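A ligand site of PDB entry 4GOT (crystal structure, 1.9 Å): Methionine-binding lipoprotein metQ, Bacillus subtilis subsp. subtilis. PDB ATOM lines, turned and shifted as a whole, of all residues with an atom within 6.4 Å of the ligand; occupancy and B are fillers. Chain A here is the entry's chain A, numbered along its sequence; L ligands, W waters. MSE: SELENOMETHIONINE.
The guanidinium group (NH2) of Arg 119 is in hydrogen-bond range of the backbone carbonyl oxygen (O) of Glu 87, 2.8 Å away.
The guanidinium group of Arg 119 lies within salt-bridge range of the side-chain carboxylate of Glu 116 (2.7 Å).
OE1 of Glu 87 sits at hydrogen-bond distance from N of Asn 180 (3.0 Å).
A ring nitrogen (NE2) of His 85 lies within hydrogen-bond range of the side-chain carboxylate (OE2) of Glu 87.
ND2 of Asn 178 lies close to OH of Tyr 43.
NE2 of His 62 lies within hydrogen-bond range of OE2 of Glu 116 (2.7 Å).
OD1 of Asn 180 is in hydrogen-bond range of OH of Tyr 43, at 2.7 Å.
The side-chain amide oxygen (OD1) of Asn 113 sits close to the backbone NH (N) of Ala 115 (3.4 Å).
Water W3 lies within hydrogen-bond range of OXT of the ligand (2.6 Å), N of Val 179 (2.9 Å) and O of Glu 87 (3.1 Å).
Water W2 lies within hydrogen-bond range of the backbone carbonyl oxygen of Phe 60 (2.6 Å), a nitrogen (N) of the ligand (2.8 Å), the side-chain hydroxyl of Thr 13 (2.9 Å) and the side-chain amide oxygen of Asn 180 (3.4 Å).
His 17 touches the ligand.
CD2 of Tyr 43 touches CE of the ligand (3.5 Å).
Phe 60 touches the ligand (O to CB, 3.3 Å).
NE2 of His 62 touches SE of the ligand, 3.2 Å away.
Tyr 65 touches the ligand (CD2 to CE, 3.5 Å).
Asn 113 touches the ligand (ND2 to SE, 3.8 Å).
OE2 of Glu 116 touches CG of the ligand, 3.6 Å away.
Hydrophobic or aromatic side chains within 4 Å of the ligand: His 17, Tyr 43, Phe 60, His 62 and Tyr 65.
Within 4 Å of the ligand: His 17, Tyr 43, Phe 60, His 62, Tyr 65, Glu 87, Asn 113, Glu 116, Arg 119, Asn 178, Asn 180 and Asn 206.
ND2 of Asn 206 lies within hydrogen-bond range of O of the ligand (2.8 Å).
The guanidinium group of Arg 119 lies within salt-bridge range of an oxygen (OXT) of the ligand, at 2.8 Å.
A nitrogen (N) of the ligand lies within salt-bridge range of the side-chain carboxylate of Glu 87 (2.9 Å).
The side-chain amide oxygen of Asn 178 sits close to an oxygen (OXT) of the ligand, 3.0 Å away.
OD1 of Asn 180 lies within hydrogen-bond range of N of the ligand (3.4 Å).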
ATOM      1  N   THR A  13      26.063  -8.386  17.467  1.00  0.00           N
ATOM      2  CA  THR A  13      27.407  -8.644  16.974  1.00  0.00           C
ATOM      3  C   THR A  13      27.258  -9.601  15.769  1.00  0.00           C
ATOM      4  O   THR A  13      26.251 -10.350  15.664  1.00  0.00           O
ATOM      5  CB  THR A  13      28.327  -9.199  18.124  1.00  0.00           C
ATOM      6  OG1 THR A  13      27.607 -10.148  18.934  1.00  0.00           O
ATOM      7  CG2 THR A  13      28.852  -8.048  19.058  1.00  0.00           C
ATOM      8  N   PRO A  16      27.949 -15.149  16.646  1.00  0.00           N
ATOM      9  CA  PRO A  16      26.800 -15.790  15.959  1.00  0.00           C
ATOM     10  C   PRO A  16      25.502 -14.994  15.940  1.00  0.00           C
ATOM     11  O   PRO A  16      24.535 -15.424  15.310  1.00  0.00           O
ATOM     12  CB  PRO A  16      26.553 -17.044  16.807  1.00  0.00           C
ATOM     13  CG  PRO A  16      26.992 -16.638  18.167  1.00  0.00           C
ATOM     14  CD  PRO A  16      28.195 -15.756  17.978  1.00  0.00           C
ATOM     15  N   HIS A  17      25.469 -13.859  16.662  1.00  0.00           N
ATOM     16  CA  HIS A  17      24.215 -13.248  17.043  1.00  0.00           C
ATOM     17  C   HIS A  17      23.412 -12.740  15.801  1.00  0.00           C
ATOM     18  O   HIS A  17      22.195 -13.054  15.675  1.00  0.00           O
ATOM     19  CB  HIS A  17      24.417 -12.113  18.074  1.00  0.00           C
ATOM     20  CG  HIS A  17      25.217 -12.489  19.272  1.00  0.00           C
ATOM     21  ND1 HIS A  17      26.538 -12.845  19.185  1.00  0.00           N
ATOM     22  CD2 HIS A  17      24.910 -12.488  20.600  1.00  0.00           C
ATOM     23  CE1 HIS A  17      26.981 -13.179  20.392  1.00  0.00           C
ATOM     24  NE2 HIS A  17      26.026 -12.927  21.273  1.00  0.00           N
ATOM     25  N   TYR A  43      31.679  -3.495  21.376  1.00  0.00           N
ATOM     26  CA  TYR A  43      30.768  -3.849  22.410  1.00  0.00           C
ATOM     27  C   TYR A  43      30.161  -2.620  23.075  1.00  0.00           C
ATOM     28  O   TYR A  43      28.999  -2.661  23.488  1.00  0.00           O
ATOM     29  CB  TYR A  43      31.519  -4.649  23.492  1.00  0.00           C
ATOM     30  CG  TYR A  43      31.831  -6.138  23.293  1.00  0.00           C
ATOM     31  CD1 TYR A  43      31.231  -6.916  22.336  1.00  0.00           C
ATOM     32  CD2 TYR A  43      32.739  -6.765  24.165  1.00  0.00           C
ATOM     33  CE1 TYR A  43      31.507  -8.289  22.224  1.00  0.00           C
ATOM     34  CE2 TYR A  43      33.038  -8.120  24.077  1.00  0.00           C
ATOM     35  CZ  TYR A  43      32.423  -8.880  23.092  1.00  0.00           C
ATOM     36  OH  TYR A  43      32.715 -10.202  23.002  1.00  0.00           O
ATOM     37  N   PHE A  60      23.983  -9.251  22.255  1.00  0.00           N
ATOM     38  CA  PHE A  60      25.460  -9.236  22.247  1.00  0.00           C
ATOM     39  C   PHE A  60      26.156  -9.523  23.581  1.00  0.00           C
ATOM     40  O   PHE A  60      27.329  -9.859  23.544  1.00  0.00           O
ATOM     41  CB  PHE A  60      26.015  -7.904  21.668  1.00  0.00           C
ATOM     42  CG  PHE A  60      26.116  -6.814  22.698  1.00  0.00           C
ATOM     43  CD1 PHE A  60      24.971  -6.231  23.218  1.00  0.00           C
ATOM     44  CD2 PHE A  60      27.355  -6.457  23.256  1.00  0.00           C
ATOM     45  CE1 PHE A  60      25.051  -5.282  24.222  1.00  0.00           C
ATOM     46  CE2 PHE A  60      27.444  -5.495  24.249  1.00  0.00           C
ATOM     47  CZ  PHE A  60      26.289  -4.899  24.720  1.00  0.00           C
ATOM     48  N   GLN A  61      25.455  -9.410  24.731  1.00  0.00           N
ATOM     49  CA  GLN A  61      26.122  -9.385  26.066  1.00  0.00           C
ATOM     50  C   GLN A  61      25.563 -10.400  27.019  1.00  0.00           C
ATOM     51  O   GLN A  61      24.536 -11.004  26.742  1.00  0.00           O
ATOM     52  CB  GLN A  61      25.930  -7.994  26.694  1.00  0.00           C
ATOM     53  CG  GLN A  61      24.517  -7.734  27.251  1.00  0.00           C
ATOM     54  CD  GLN A  61      24.169  -6.273  27.383  1.00  0.00           C
ATOM     55  OE1 GLN A  61      24.893  -5.507  28.024  1.00  0.00           O
ATOM     56  NE2 GLN A  61      23.035  -5.869  26.777  1.00  0.00           N
ATOM     57  N   HIS A  62      26.170 -10.515  28.185  1.00  0.00           N
ATOM     58  CA  HIS A  62      25.622 -11.336  29.289  1.00  0.00           C
ATOM     59  C   HIS A  62      25.179 -10.399  30.428  1.00  0.00           C
ATOM     60  O   HIS A  62      25.376  -9.192  30.346  1.00  0.00           O
ATOM     61  CB  HIS A  62      26.634 -12.390  29.785  1.00  0.00           C
ATOM     62  CG  HIS A  62      28.049 -11.892  29.860  1.00  0.00           C
ATOM     63  ND1 HIS A  62      28.491 -10.941  30.767  1.00  0.00           N
ATOM     64  CD2 HIS A  62      29.144 -12.243  29.136  1.00  0.00           C
ATOM     65  CE1 HIS A  62      29.781 -10.714  30.587  1.00  0.00           C
ATOM     66  NE2 HIS A  62      30.195 -11.466  29.568  1.00  0.00           N
ATOM     67  N   TYR A  65      27.864  -8.202  32.090  1.00  0.00           N
ATOM     68  CA  TYR A  65      28.263  -7.089  31.252  1.00  0.00           C
ATOM     69  C   TYR A  65      27.228  -5.949  31.360  1.00  0.00           C
ATOM     70  O   TYR A  65      27.571  -4.782  31.492  1.00  0.00           O
ATOM     71  CB  TYR A  65      28.440  -7.519  29.800  1.00  0.00           C
ATOM     72  CG  TYR A  65      29.073  -6.407  28.960  1.00  0.00           C
ATOM     73  CD1 TYR A  65      28.290  -5.485  28.336  1.00  0.00           C
ATOM     74  CD2 TYR A  65      30.458  -6.300  28.813  1.00  0.00           C
ATOM     75  CE1 TYR A  65      28.838  -4.449  27.598  1.00  0.00           C
ATOM     76  CE2 TYR A  65      31.027  -5.264  28.076  1.00  0.00           C
ATOM     77  CZ  TYR A  65      30.209  -4.338  27.462  1.00  0.00           C
ATOM     78  OH  TYR A  65      30.730  -3.321  26.676  1.00  0.00           O
ATOM     79  N   HIS A  85      21.623 -18.158  24.595  1.00  0.00           N
ATOM     80  CA  HIS A  85      22.793 -18.988  24.293  1.00  0.00           C
ATOM     81  C   HIS A  85      24.001 -18.622  25.194  1.00  0.00           C
ATOM     82  O   HIS A  85      24.161 -17.494  25.673  1.00  0.00           O
ATOM     83  CB  HIS A  85      23.165 -18.917  22.786  1.00  0.00           C
ATOM     84  CG  HIS A  85      24.034 -17.753  22.407  1.00  0.00           C
ATOM     85  ND1 HIS A  85      23.575 -16.686  21.658  1.00  0.00           N
ATOM     86  CD2 HIS A  85      25.360 -17.525  22.602  1.00  0.00           C
ATOM     87  CE1 HIS A  85      24.556 -15.844  21.452  1.00  0.00           C
ATOM     88  NE2 HIS A  85      25.652 -16.324  22.005  1.00  0.00           N
ATOM     89  N   LEU A  86      24.856 -19.610  25.353  1.00  0.00           N
ATOM     90  CA  LEU A  86      26.144 -19.513  26.047  1.00  0.00           C
ATOM     91  C   LEU A  86      27.330 -19.675  25.034  1.00  0.00           C
ATOM     92  O   LEU A  86      27.288 -20.501  24.084  1.00  0.00           O
ATOM     93  CB  LEU A  86      26.183 -20.623  27.150  1.00  0.00           C
ATOM     94  CG  LEU A  86      27.412 -20.682  28.091  1.00  0.00           C
ATOM     95  CD1 LEU A  86      27.638 -19.360  28.823  1.00  0.00           C
ATOM     96  CD2 LEU A  86      27.357 -21.866  29.074  1.00  0.00           C
ATOM     97  N   GLU A  87      28.401 -18.917  25.262  1.00  0.00           N
ATOM     98  CA  GLU A  87      29.655 -19.050  24.510  1.00  0.00           C
ATOM     99  C   GLU A  87      30.813 -19.350  25.497  1.00  0.00           C
ATOM    100  O   GLU A  87      31.421 -18.431  26.013  1.00  0.00           O
ATOM    101  CB  GLU A  87      29.977 -17.745  23.774  1.00  0.00           C
ATOM    102  CG  GLU A  87      29.048 -17.391  22.649  1.00  0.00           C
ATOM    103  CD  GLU A  87      29.275 -15.968  22.128  1.00  0.00           C
ATOM    104  OE1 GLU A  87      30.396 -15.428  22.198  1.00  0.00           O
ATOM    105  OE2 GLU A  87      28.276 -15.393  21.652  1.00  0.00           O
ATOM    106  N   PRO A  88      31.083 -20.628  25.800  1.00  0.00           N
ATOM    107  CA  PRO A  88      32.259 -20.874  26.650  1.00  0.00           C
ATOM    108  C   PRO A  88      33.560 -20.205  26.117  1.00  0.00           C
ATOM    109  O   PRO A  88      33.966 -20.390  24.952  1.00  0.00           O
ATOM    110  CB  PRO A  88      32.345 -22.394  26.676  1.00  0.00           C
ATOM    111  CG  PRO A  88      30.929 -22.819  26.541  1.00  0.00           C
ATOM    112  CD  PRO A  88      30.338 -21.865  25.537  1.00  0.00           C
ATOM    113  N   PHE A  89      34.140 -19.359  26.992  1.00  0.00           N
ATOM    114  CA  PHE A  89      35.338 -18.569  26.762  1.00  0.00           C
ATOM    115  C   PHE A  89      36.547 -19.459  26.406  1.00  0.00           C
ATOM    116  O   PHE A  89      36.710 -20.598  26.920  1.00  0.00           O
ATOM    117  CB  PHE A  89      35.653 -17.819  28.072  1.00  0.00           C
ATOM    118  CG  PHE A  89      36.187 -16.420  27.917  1.00  0.00           C
ATOM    119  CD1 PHE A  89      36.298 -15.782  26.698  1.00  0.00           C
ATOM    120  CD2 PHE A  89      36.502 -15.710  29.053  1.00  0.00           C
ATOM    121  CE1 PHE A  89      36.765 -14.480  26.599  1.00  0.00           C
ATOM    122  CE2 PHE A  89      36.953 -14.388  28.963  1.00  0.00           C
ATOM    123  CZ  PHE A  89      37.085 -13.771  27.722  1.00  0.00           C
ATOM    124  N   ASN A 113      37.639  -5.820  28.850  1.00  0.00           N
ATOM    125  CA  ASN A 113      36.228  -5.899  29.259  1.00  0.00           C
ATOM    126  C   ASN A 113      36.158  -5.996  30.796  1.00  0.00           C
ATOM    127  O   ASN A 113      36.385  -7.078  31.366  1.00  0.00           O
ATOM    128  CB  ASN A 113      35.614  -7.165  28.577  1.00  0.00           C
ATOM    129  CG  ASN A 113      34.116  -7.295  28.718  1.00  0.00           C
ATOM    130  OD1 ASN A 113      33.496  -6.852  29.684  1.00  0.00           O
ATOM    131  ND2 ASN A 113      33.518  -7.928  27.718  1.00  0.00           N
ATOM    132  N   ALA A 115      33.782  -6.034  33.004  1.00  0.00           N
ATOM    133  CA  ALA A 115      32.834  -7.055  33.461  1.00  0.00           C
ATOM    134  C   ALA A 115      33.337  -8.498  33.404  1.00  0.00           C
ATOM    135  O   ALA A 115      32.871  -9.364  34.168  1.00  0.00           O
ATOM    136  CB  ALA A 115      31.545  -6.935  32.665  1.00  0.00           C
ATOM    137  N   GLU A 116      34.287  -8.776  32.505  1.00  0.00           N
ATOM    138  CA  GLU A 116      34.777 -10.140  32.330  1.00  0.00           C
ATOM    139  C   GLU A 116      36.127 -10.420  33.012  1.00  0.00           C
ATOM    140  O   GLU A 116      36.712 -11.450  32.780  1.00  0.00           O
ATOM    141  CB  GLU A 116      34.894 -10.479  30.842  1.00  0.00           C
ATOM    142  CG  GLU A 116      33.525 -10.619  30.185  1.00  0.00           C
ATOM    143  CD  GLU A 116      33.567 -11.443  28.918  1.00  0.00           C
ATOM    144  OE1 GLU A 116      34.556 -11.298  28.161  1.00  0.00           O
ATOM    145  OE2 GLU A 116      32.601 -12.243  28.699  1.00  0.00           O
ATOM    146  N   ARG A 119      35.841 -13.583  34.989  1.00  0.00           N
ATOM    147  CA  ARG A 119      35.628 -14.742  34.082  1.00  0.00           C
ATOM    148  C   ARG A 119      36.980 -15.300  33.566  1.00  0.00           C
ATOM    149  O   ARG A 119      37.227 -16.476  33.589  1.00  0.00           O
ATOM    150  CB  ARG A 119      34.750 -14.321  32.901  1.00  0.00           C
ATOM    151  CG  ARG A 119      34.273 -15.448  32.023  1.00  0.00           C
ATOM    152  CD  ARG A 119      33.459 -14.938  30.845  1.00  0.00           C
ATOM    153  NE  ARG A 119      32.870 -16.082  30.151  1.00  0.00           N
ATOM    154  CZ  ARG A 119      32.202 -16.013  28.999  1.00  0.00           C
ATOM    155  NH1 ARG A 119      32.000 -14.860  28.357  1.00  0.00           N
ATOM    156  NH2 ARG A 119      31.743 -17.151  28.468  1.00  0.00           N
ATOM    157  N   ASN A 178      36.819 -13.958  23.073  1.00  0.00           N
ATOM    158  CA  ASN A 178      35.396 -14.256  23.210  1.00  0.00           C
ATOM    159  C   ASN A 178      34.977 -15.045  21.973  1.00  0.00           C
ATOM    160  O   ASN A 178      35.418 -14.700  20.875  1.00  0.00           O
ATOM    161  CB  ASN A 178      34.566 -12.962  23.239  1.00  0.00           C
ATOM    162  CG  ASN A 178      34.806 -12.102  24.485  1.00  0.00           C
ATOM    163  OD1 ASN A 178      34.182 -12.311  25.524  1.00  0.00           O
ATOM    164  ND2 ASN A 178      35.721 -11.166  24.384  1.00  0.00           N
ATOM    165  N   VAL A 179      34.118 -16.050  22.117  1.00  0.00           N
ATOM    166  CA  VAL A 179      33.698 -16.876  20.962  1.00  0.00           C
ATOM    167  C   VAL A 179      33.203 -16.027  19.758  1.00  0.00           C
ATOM    168  O   VAL A 179      33.546 -16.323  18.622  1.00  0.00           O
ATOM    169  CB  VAL A 179      32.626 -17.920  21.350  1.00  0.00           C
ATOM    170  CG1 VAL A 179      32.126 -18.657  20.083  1.00  0.00           C
ATOM    171  CG2 VAL A 179      33.113 -18.901  22.443  1.00  0.00           C
ATOM    172  N   ASN A 180      32.403 -14.987  19.985  1.00  0.00           N
ATOM    173  CA  ASN A 180      31.916 -14.175  18.837  1.00  0.00           C
ATOM    174  C   ASN A 180      33.025 -13.578  17.950  1.00  0.00           C
ATOM    175  O   ASN A 180      32.971 -13.634  16.711  1.00  0.00           O
ATOM    176  CB  ASN A 180      30.938 -13.075  19.276  1.00  0.00           C
ATOM    177  CG  ASN A 180      31.600 -11.892  19.975  1.00  0.00           C
ATOM    178  OD1 ASN A 180      31.956 -11.967  21.176  1.00  0.00           O
ATOM    179  ND2 ASN A 180      31.678 -10.747  19.258  1.00  0.00           N
ATOM    180  N   TYR A 204      27.323 -16.657  32.328  1.00  0.00           N
ATOM    181  CA  TYR A 204      27.621 -15.757  31.214  1.00  0.00           C
ATOM    182  C   TYR A 204      26.802 -16.009  29.940  1.00  0.00           C
ATOM    183  O   TYR A 204      27.208 -15.613  28.814  1.00  0.00           O
ATOM    184  CB  TYR A 204      29.174 -15.696  30.934  1.00  0.00           C
ATOM    185  CG  TYR A 204      29.999 -15.228  32.146  1.00  0.00           C
ATOM    186  CD1 TYR A 204      30.081 -13.876  32.492  1.00  0.00           C
ATOM    187  CD2 TYR A 204      30.676 -16.147  32.964  1.00  0.00           C
ATOM    188  CE1 TYR A 204      30.800 -13.448  33.595  1.00  0.00           C
ATOM    189  CE2 TYR A 204      31.399 -15.729  34.076  1.00  0.00           C
ATOM    190  CZ  TYR A 204      31.454 -14.378  34.397  1.00  0.00           C
ATOM    191  OH  TYR A 204      32.188 -13.954  35.490  1.00  0.00           O
ATOM    192  N   ALA A 205      25.596 -16.545  30.102  1.00  0.00           N
ATOM    193  CA  ALA A 205      24.695 -16.670  28.958  1.00  0.00           C
ATOM    194  C   ALA A 205      24.443 -15.301  28.345  1.00  0.00           C
ATOM    195  O   ALA A 205      24.255 -14.287  29.053  1.00  0.00           O
ATOM    196  CB  ALA A 205      23.378 -17.306  29.387  1.00  0.00           C
ATOM    197  N   ASN A 206      24.394 -15.261  27.026  1.00  0.00           N
ATOM    198  CA  ASN A 206      24.091 -14.032  26.309  1.00  0.00           C
ATOM    199  C   ASN A 206      22.569 -13.837  26.234  1.00  0.00           C
ATOM    200  O   ASN A 206      21.821 -14.806  26.126  1.00  0.00           O
ATOM    201  CB  ASN A 206      24.655 -14.089  24.881  1.00  0.00           C
ATOM    202  CG  ASN A 206      26.173 -13.880  24.817  1.00  0.00           C
ATOM    203  OD1 ASN A 206      26.641 -13.288  23.891  1.00  0.00           O
ATOM    204  ND2 ASN A 206      26.932 -14.350  25.846  1.00  0.00           N
HETATM  205  N   MSE L   1      29.411 -12.892  23.200  1.00  0.00           N
HETATM  206  CA  MSE L   1      30.399 -12.566  24.267  1.00  0.00           C
HETATM  207  C   MSE L   1      30.671 -13.763  25.230  1.00  0.00           C
HETATM  208  O   MSE L   1      29.716 -14.320  25.692  1.00  0.00           O
HETATM  209  OXT MSE L   1      31.791 -14.184  25.603  1.00  0.00           O
HETATM  210  CB  MSE L   1      29.863 -11.385  25.087  1.00  0.00           C
HETATM  211  CG  MSE L   1      30.837 -10.735  26.003  1.00  0.00           C
HETATM  212 SE   MSE L   1      30.013  -9.365  27.178  1.00  0.00          SE
HETATM  213  CE  MSE L   1      29.820  -7.845  25.750  1.00  0.00           C
HETATM  214  O   HOH W   1      28.864 -16.697  27.013  1.00  0.00           O
HETATM  215  O   HOH W   2      28.784 -10.705  21.550  1.00  0.00           O
HETATM  216  O   HOH W   3      33.155 -16.214  24.812  1.00  0.00           O
